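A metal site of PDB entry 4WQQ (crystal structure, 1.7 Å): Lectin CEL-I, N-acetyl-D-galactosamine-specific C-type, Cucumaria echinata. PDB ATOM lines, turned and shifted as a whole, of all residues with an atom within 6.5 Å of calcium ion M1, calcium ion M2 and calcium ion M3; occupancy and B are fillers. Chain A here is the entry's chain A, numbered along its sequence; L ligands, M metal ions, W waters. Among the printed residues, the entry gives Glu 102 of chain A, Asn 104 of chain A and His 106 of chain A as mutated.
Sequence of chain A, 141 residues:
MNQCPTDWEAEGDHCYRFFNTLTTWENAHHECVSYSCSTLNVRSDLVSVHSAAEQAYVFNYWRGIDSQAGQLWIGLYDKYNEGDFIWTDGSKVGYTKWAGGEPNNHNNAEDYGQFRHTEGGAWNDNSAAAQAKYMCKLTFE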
ATOM      1  N   ASP A  78     -20.211 -16.548  -2.341  1.00  0.00           N
ATOM      2  CA  ASP A  78     -20.246 -17.961  -2.738  1.00  0.00           C
ATOM      3  C   ASP A  78     -20.905 -18.202  -4.107  1.00  0.00           C
ATOM      4  O   ASP A  78     -21.597 -19.198  -4.324  1.00  0.00           O
ATOM      5  CB  ASP A  78     -20.920 -18.799  -1.646  1.00  0.00           C
ATOM      6  CG  ASP A  78     -22.459 -18.626  -1.588  1.00  0.00           C
ATOM      7  OD1 ASP A  78     -23.000 -17.576  -1.909  1.00  0.00           O
ATOM      8  OD2 ASP A  78     -23.151 -19.550  -1.171  1.00  0.00           O
ATOM      9  N   LYS A  79     -20.700 -17.245  -5.004  1.00  0.00           N
ATOM     10  CA  LYS A  79     -21.100 -17.327  -6.384  1.00  0.00           C
ATOM     11  C   LYS A  79     -20.594 -18.601  -7.068  1.00  0.00           C
ATOM     12  O   LYS A  79     -21.337 -19.232  -7.772  1.00  0.00           O
ATOM     13  CB  LYS A  79     -20.584 -16.117  -7.185  1.00  0.00           C
ATOM     14  CG  LYS A  79     -20.976 -16.160  -8.627  1.00  0.00           C
ATOM     15  CD  LYS A  79     -20.531 -14.956  -9.461  1.00  0.00           C
ATOM     16  CE  LYS A  79     -20.703 -15.360 -10.938  1.00  0.00           C
ATOM     17  NZ  LYS A  79     -20.848 -14.163 -11.780  1.00  0.00           N
ATOM     18  N   GLU A  82     -21.609 -22.517  -4.231  1.00  0.00           N
ATOM     19  CA  GLU A  82     -22.658 -22.284  -3.257  1.00  0.00           C
ATOM     20  C   GLU A  82     -22.402 -22.957  -1.933  1.00  0.00           C
ATOM     21  O   GLU A  82     -22.201 -24.185  -1.867  1.00  0.00           O
ATOM     22  CB  GLU A  82     -24.024 -22.698  -3.821  1.00  0.00           C
ATOM     23  CG  GLU A  82     -25.247 -22.579  -2.896  1.00  0.00           C
ATOM     24  CD  GLU A  82     -25.509 -21.156  -2.444  1.00  0.00           C
ATOM     25  OE1 GLU A  82     -25.779 -20.986  -1.225  1.00  0.00           O
ATOM     26  OE2 GLU A  82     -25.375 -20.256  -3.295  1.00  0.00           O
ATOM     27  N   GLY A  83     -22.486 -22.181  -0.854  1.00  0.00           N
ATOM     28  CA  GLY A  83     -22.267 -22.707   0.497  1.00  0.00           C
ATOM     29  C   GLY A  83     -20.815 -22.686   0.898  1.00  0.00           C
ATOM     30  O   GLY A  83     -20.526 -22.820   2.102  1.00  0.00           O
ATOM     31  N   PHE A  85     -18.065 -20.130   0.982  1.00  0.00           N
ATOM     32  CA  PHE A  85     -17.700 -18.724   0.814  1.00  0.00           C
ATOM     33  C   PHE A  85     -16.209 -18.575   0.669  1.00  0.00           C
ATOM     34  O   PHE A  85     -15.463 -19.298   1.313  1.00  0.00           O
ATOM     35  CB  PHE A  85     -18.252 -17.885   1.976  1.00  0.00           C
ATOM     36  CG  PHE A  85     -19.752 -17.595   1.832  1.00  0.00           C
ATOM     37  CD1 PHE A  85     -20.689 -18.501   2.249  1.00  0.00           C
ATOM     38  CD2 PHE A  85     -20.217 -16.435   1.204  1.00  0.00           C
ATOM     39  CE1 PHE A  85     -22.051 -18.258   2.082  1.00  0.00           C
ATOM     40  CE2 PHE A  85     -21.548 -16.180   1.039  1.00  0.00           C
ATOM     41  CZ  PHE A  85     -22.485 -17.130   1.454  1.00  0.00           C
ATOM     42  N   GLY A 101     -28.510 -18.179  12.333  1.00  0.00           N
ATOM     43  CA  GLY A 101     -29.173 -18.680  11.124  1.00  0.00           C
ATOM     44  C   GLY A 101     -28.628 -18.319   9.760  1.00  0.00           C
ATOM     45  O   GLY A 101     -29.181 -18.748   8.726  1.00  0.00           O
ATOM     46  N   GLU A 102     -27.492 -17.597   9.748  1.00  0.00           N
ATOM     47  CA  GLU A 102     -26.822 -17.289   8.481  1.00  0.00           C
ATOM     48  C   GLU A 102     -25.593 -18.222   8.319  1.00  0.00           C
ATOM     49  O   GLU A 102     -25.038 -18.672   9.364  1.00  0.00           O
ATOM     50  CB  GLU A 102     -26.383 -15.829   8.532  1.00  0.00           C
ATOM     51  CG  GLU A 102     -27.528 -14.900   8.874  1.00  0.00           C
ATOM     52  CD  GLU A 102     -28.682 -14.834   7.848  1.00  0.00           C
ATOM     53  OE1 GLU A 102     -28.497 -15.306   6.714  1.00  0.00           O
ATOM     54  OE2 GLU A 102     -29.795 -14.281   8.168  1.00  0.00           O
ATOM     55  N   PRO A 103     -25.133 -18.451   7.084  1.00  0.00           N
ATOM     56  CA  PRO A 103     -25.744 -17.912   5.819  1.00  0.00           C
ATOM     57  C   PRO A 103     -26.959 -18.758   5.466  1.00  0.00           C
ATOM     58  O   PRO A 103     -26.928 -19.952   5.668  1.00  0.00           O
ATOM     59  CB  PRO A 103     -24.645 -18.134   4.776  1.00  0.00           C
ATOM     60  CG  PRO A 103     -23.837 -19.248   5.291  1.00  0.00           C
ATOM     61  CD  PRO A 103     -23.904 -19.190   6.797  1.00  0.00           C
ATOM     62  N   ASN A 104     -28.052 -18.171   5.068  1.00  0.00           N
ATOM     63  CA  ASN A 104     -29.226 -18.959   4.779  1.00  0.00           C
ATOM     64  C   ASN A 104     -29.604 -19.013   3.323  1.00  0.00           C
ATOM     65  O   ASN A 104     -30.611 -19.599   3.002  1.00  0.00           O
ATOM     66  CB  ASN A 104     -30.385 -18.459   5.613  1.00  0.00           C
ATOM     67  CG  ASN A 104     -30.846 -17.061   5.263  1.00  0.00           C
ATOM     68  OD1 ASN A 104     -30.216 -16.344   4.509  1.00  0.00           O
ATOM     69  ND2 ASN A 104     -31.934 -16.650   5.845  1.00  0.00           N
ATOM     70  N   ASN A 105     -28.840 -18.379   2.427  1.00  0.00           N
ATOM     71  CA  ASN A 105     -29.110 -18.429   0.979  1.00  0.00           C
ATOM     72  C   ASN A 105     -30.591 -18.165   0.702  1.00  0.00           C
ATOM     73  O   ASN A 105     -31.243 -18.870  -0.076  1.00  0.00           O
ATOM     74  CB  ASN A 105     -28.635 -19.769   0.387  1.00  0.00           C
ATOM     75  CG  ASN A 105     -28.454 -19.703  -1.091  1.00  0.00           C
ATOM     76  OD1 ASN A 105     -27.887 -18.735  -1.684  1.00  0.00           O
ATOM     77  ND2 ASN A 105     -28.926 -20.739  -1.760  1.00  0.00           N
ATOM     78  N   HIS A 106     -31.110 -17.110   1.328  1.00  0.00           N
ATOM     79  CA  HIS A 106     -32.562 -16.934   1.372  1.00  0.00           C
ATOM     80  C   HIS A 106     -33.131 -16.881  -0.033  1.00  0.00           C
ATOM     81  O   HIS A 106     -32.532 -16.341  -0.978  1.00  0.00           O
ATOM     82  CB  HIS A 106     -32.918 -15.657   2.119  1.00  0.00           C
ATOM     83  CG  HIS A 106     -34.382 -15.436   2.249  1.00  0.00           C
ATOM     84  ND1 HIS A 106     -35.127 -16.100   3.184  1.00  0.00           N
ATOM     85  CD2 HIS A 106     -35.221 -14.603   1.601  1.00  0.00           C
ATOM     86  CE1 HIS A 106     -36.382 -15.689   3.123  1.00  0.00           C
ATOM     87  NE2 HIS A 106     -36.468 -14.805   2.144  1.00  0.00           N
ATOM     88  N   ASN A 108     -32.990 -19.016  -2.195  1.00  0.00           N
ATOM     89  CA  ASN A 108     -32.016 -19.578  -3.073  1.00  0.00           C
ATOM     90  C   ASN A 108     -31.175 -18.600  -3.863  1.00  0.00           C
ATOM     91  O   ASN A 108     -30.714 -18.964  -4.929  1.00  0.00           O
ATOM     92  CB  ASN A 108     -32.643 -20.542  -4.110  1.00  0.00           C
ATOM     93  CG  ASN A 108     -33.188 -21.764  -3.470  1.00  0.00           C
ATOM     94  OD1 ASN A 108     -32.557 -22.817  -3.469  1.00  0.00           O
ATOM     95  ND2 ASN A 108     -34.359 -21.654  -2.916  1.00  0.00           N
ATOM     96  N   ALA A 109     -30.949 -17.387  -3.346  1.00  0.00           N
ATOM     97  CA  ALA A 109     -30.394 -16.288  -4.101  1.00  0.00           C
ATOM     98  C   ALA A 109     -29.649 -15.290  -3.253  1.00  0.00           C
ATOM     99  O   ALA A 109     -29.931 -14.110  -3.315  1.00  0.00           O
ATOM    100  CB  ALA A 109     -31.510 -15.557  -4.829  1.00  0.00           C
ATOM    101  N   GLU A 110     -28.775 -15.769  -2.385  1.00  0.00           N
ATOM    102  CA  GLU A 110     -27.973 -14.873  -1.587  1.00  0.00           C
ATOM    103  C   GLU A 110     -26.559 -15.380  -1.607  1.00  0.00           C
ATOM    104  O   GLU A 110     -26.199 -16.374  -0.922  1.00  0.00           O
ATOM    105  CB  GLU A 110     -28.509 -14.724  -0.154  1.00  0.00           C
ATOM    106  CG  GLU A 110     -29.874 -14.056  -0.055  1.00  0.00           C
ATOM    107  CD  GLU A 110     -30.223 -13.673   1.371  1.00  0.00           C
ATOM    108  OE1 GLU A 110     -29.935 -14.511   2.281  1.00  0.00           O
ATOM    109  OE2 GLU A 110     -30.817 -12.576   1.596  1.00  0.00           O
ATOM    110  N   ASP A 111     -25.720 -14.646  -2.352  1.00  0.00           N
ATOM    111  CA  ASP A 111     -24.352 -15.037  -2.513  1.00  0.00           C
ATOM    112  C   ASP A 111     -23.291 -14.046  -1.962  1.00  0.00           C
ATOM    113  O   ASP A 111     -22.123 -14.214  -2.196  1.00  0.00           O
ATOM    114  CB  ASP A 111     -24.064 -15.391  -3.977  1.00  0.00           C
ATOM    115  CG  ASP A 111     -24.792 -16.694  -4.472  1.00  0.00           C
ATOM    116  OD1 ASP A 111     -25.463 -17.451  -3.684  1.00  0.00           O
ATOM    117  OD2 ASP A 111     -24.660 -16.968  -5.701  1.00  0.00           O
ATOM    118  N   TYR A 112     -23.702 -13.004  -1.268  1.00  0.00           N
ATOM    119  CA  TYR A 112     -22.835 -11.837  -1.004  1.00  0.00           C
ATOM    120  C   TYR A 112     -22.848 -11.489   0.462  1.00  0.00           C
ATOM    121  O   TYR A 112     -23.907 -11.225   1.047  1.00  0.00           O
ATOM    122  CB  TYR A 112     -23.196 -10.627  -1.934  1.00  0.00           C
ATOM    123  CG  TYR A 112     -23.163 -11.074  -3.332  1.00  0.00           C
ATOM    124  CD1 TYR A 112     -21.930 -11.312  -3.963  1.00  0.00           C
ATOM    125  CD2 TYR A 112     -24.341 -11.479  -3.987  1.00  0.00           C
ATOM    126  CE1 TYR A 112     -21.865 -11.845  -5.222  1.00  0.00           C
ATOM    127  CE2 TYR A 112     -24.273 -12.023  -5.266  1.00  0.00           C
ATOM    128  CZ  TYR A 112     -23.045 -12.177  -5.872  1.00  0.00           C
ATOM    129  OH  TYR A 112     -23.011 -12.741  -7.162  1.00  0.00           O
ATOM    130  N   ARG A 116     -24.080  -6.962   9.504  1.00  0.00           N
ATOM    131  CA  ARG A 116     -25.179  -6.237  10.145  1.00  0.00           C
ATOM    132  C   ARG A 116     -24.652  -5.096  11.022  1.00  0.00           C
ATOM    133  O   ARG A 116     -23.502  -5.102  11.427  1.00  0.00           O
ATOM    134  CB  ARG A 116     -25.958  -7.235  11.050  1.00  0.00           C
ATOM    135  CG  ARG A 116     -26.421  -8.381  10.217  1.00  0.00           C
ATOM    136  CD  ARG A 116     -27.648  -9.052  10.696  1.00  0.00           C
ATOM    137  NE  ARG A 116     -28.655  -8.868   9.647  1.00  0.00           N
ATOM    138  CZ  ARG A 116     -29.386  -9.843   9.086  1.00  0.00           C
ATOM    139  NH1 ARG A 116     -29.297 -11.172   9.452  1.00  0.00           N
ATOM    140  NH2 ARG A 116     -30.234  -9.484   8.133  1.00  0.00           N
ATOM    141  N   ASN A 124     -24.246 -11.528   7.469  1.00  0.00           N
ATOM    142  CA  ASN A 124     -25.357 -12.050   6.727  1.00  0.00           C
ATOM    143  C   ASN A 124     -24.946 -12.204   5.244  1.00  0.00           C
ATOM    144  O   ASN A 124     -24.103 -11.440   4.745  1.00  0.00           O
ATOM    145  CB  ASN A 124     -26.477 -11.062   6.816  1.00  0.00           C
ATOM    146  CG  ASN A 124     -27.676 -11.483   6.029  1.00  0.00           C
ATOM    147  OD1 ASN A 124     -28.107 -12.635   6.048  1.00  0.00           O
ATOM    148  ND2 ASN A 124     -28.211 -10.535   5.267  1.00  0.00           N
ATOM    149  N   ASP A 125     -25.519 -13.193   4.571  1.00  0.00           N
ATOM    150  CA  ASP A 125     -25.511 -13.283   3.134  1.00  0.00           C
ATOM    151  C   ASP A 125     -26.735 -12.557   2.559  1.00  0.00           C
ATOM    152  O   ASP A 125     -27.867 -12.666   3.080  1.00  0.00           O
ATOM    153  CB  ASP A 125     -25.371 -14.726   2.626  1.00  0.00           C
ATOM    154  CG  ASP A 125     -26.528 -15.653   3.086  1.00  0.00           C
ATOM    155  OD1 ASP A 125     -27.267 -15.362   4.076  1.00  0.00           O
ATOM    156  OD2 ASP A 125     -26.646 -16.704   2.483  1.00  0.00           O
ATOM    157  N   ASN A 126     -26.505 -11.872   1.452  1.00  0.00           N
ATOM    158  CA  ASN A 126     -27.595 -11.154   0.831  1.00  0.00           C
ATOM    159  C   ASN A 126     -27.465 -11.282  -0.707  1.00  0.00           C
ATOM    160  O   ASN A 126     -26.520 -11.894  -1.246  1.00  0.00           O
ATOM    161  CB  ASN A 126     -27.628  -9.706   1.346  1.00  0.00           C
ATOM    162  CG  ASN A 126     -29.049  -9.131   1.460  1.00  0.00           C
ATOM    163  OD1 ASN A 126     -29.925  -9.418   0.632  1.00  0.00           O
ATOM    164  ND2 ASN A 126     -29.290  -8.283   2.490  1.00  0.00           N
HETATM  165  C1  LIG L   1     -33.796 -11.281   6.576  1.00  0.00           C
HETATM  166  C2  LIG L   1     -32.992 -12.532   6.813  1.00  0.00           C
HETATM  167  C3  LIG L   1     -31.633 -12.491   6.124  1.00  0.00           C
HETATM  168  C4  LIG L   1     -31.816 -12.010   4.699  1.00  0.00           C
HETATM  169  C5  LIG L   1     -32.400 -10.574   4.769  1.00  0.00           C
HETATM  170  C6  LIG L   1     -32.580  -9.840   3.469  1.00  0.00           C
HETATM  171  O1  LIG L   1     -33.176 -10.344   7.422  1.00  0.00           O
HETATM  172  O2  LIG L   1     -33.770 -13.534   6.200  1.00  0.00           O
HETATM  173  O3  LIG L   1     -31.134 -13.829   6.114  1.00  0.00           O
HETATM  174  O4  LIG L   1     -30.538 -12.055   4.092  1.00  0.00           O
HETATM  175  O5  LIG L   1     -33.782 -10.777   5.233  1.00  0.00           O
HETATM  176  O6  LIG L   1     -33.288 -10.824   2.750  1.00  0.00           O
HETATM  177 CA    CA M   1     -25.333 -18.477  -1.518  1.00  0.00          CA
HETATM  178 CA    CA M   2     -29.169 -14.165   4.559  1.00  0.00          CA
HETATM  179 CA    CA M   3     -25.833 -19.119  -5.387  1.00  0.00          CA
HETATM  180  O   HOH W   1     -25.504 -18.502   0.823  1.00  0.00           O
HETATM  181  O   HOH W   2     -28.043 -19.131  -4.297  1.00  0.00           O
HETATM  182  O   HOH W   3     -23.776 -20.001  -5.844  1.00  0.00           O
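Two residues have an atom within 4 Å of calcium ion M3: Glu 82 and Asp 111.
The backbone NH of Asn 105 lies within hydrogen-bond range of the side-chain carboxylate of Asp 125, at 2.8 Å.
The side-chain carboxylate (OE2) of Glu 110 lies close to the side-chain amide oxygen (OD1) of Asn 126.
The side-chain carboxylate (OE1) of Glu 110 lies close to the backbone NH (N) of His 106.
O of Asn 126 lies within hydrogen-bond range of N of Asp 111, at 3.1 Å.
The side-chain amide oxygen (OD1) of Asn 104 lies close to the backbone NH (N) of His 106 (3.4 Å).
The backbone NH (N) of Gly 83 lies close to the side-chain carboxylate (OD2) of Asp 78 (2.7 Å).
The guanidinium group (NH1) of Arg 116 lies within salt-bridge range of the side-chain carboxylate (OE2) of Glu 102 (3.4 Å).
Of the 20 residues printed, 5 come within 4 Å of calcium ion M1.
The nearest printed residue that does not touch calcium ion M1 is Phe 85 (4.3 Å).
Calcium ion M1 is bound by water W1 (2.3 Å), the backbone carbonyl oxygen (O) of Glu 110 (2.4 Å), the side-chain carboxylate (OD1) of Asp 111 (2.4 Å), the side-chain carboxylate (OD2) of Asp 78 (2.5 Å), the side-chain carboxylate (OE2) of Glu 82 (2.5 Å), the side-chain carboxylate (OD1) of Asp 78 (2.5 Å), the side-chain carboxylate (OE1) of Glu 82 (2.6 Å) and the side-chain amide oxygen (OD1) of Asn 105 (2.6 Å).
Calcium ion M1 has eight donor atoms within binding distance.
Five residues have an atom within 4 Å of calcium ion M2: Glu 102, Asn 104, Glu 110, Asn 124 and Asp 125.
Along chain A the residues within 4 Å of calcium ion M2 span positions 102 to 125.
The guanidinium group of Arg 116 is in hydrogen-bond range of an oxygen (O1) of the ligand (3.1 Å).
Water W2 bridges the backbone carbonyl oxygen of Asn 108 and the side-chain amide nitrogen of Asn 105.
Calcium ion M3 is bound by water W3 (2.3 Å), OD1 of Asp 111 (2.4 Å), OE2 of Glu 82 (2.4 Å), water W2 (2.5 Å) and OD2 of Asp 111 (2.5 Å).
The side-chain carboxylate (OD1) of Asp 125 binds calcium ion M2 (2.3 Å).
Calcium ion M2 is bound by OD1 of Asn 124 (2.4 Å).
The side-chain amide oxygen (OD1) of Asn 104 is bound to calcium ion M2.
OE1 of Glu 110 binds calcium ion M2, 2.4 Å away.
Calcium ion M2 is bound by O of Asp 125.
Calcium ion M2 is bound by O3 of the ligand (2.5 Å).
The side-chain carboxylate (OE1) of Glu 102 is bound to calcium ion M2 (2.5 Å).
Calcium ion M2 is bound by O4 of the ligand (2.6 Å).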
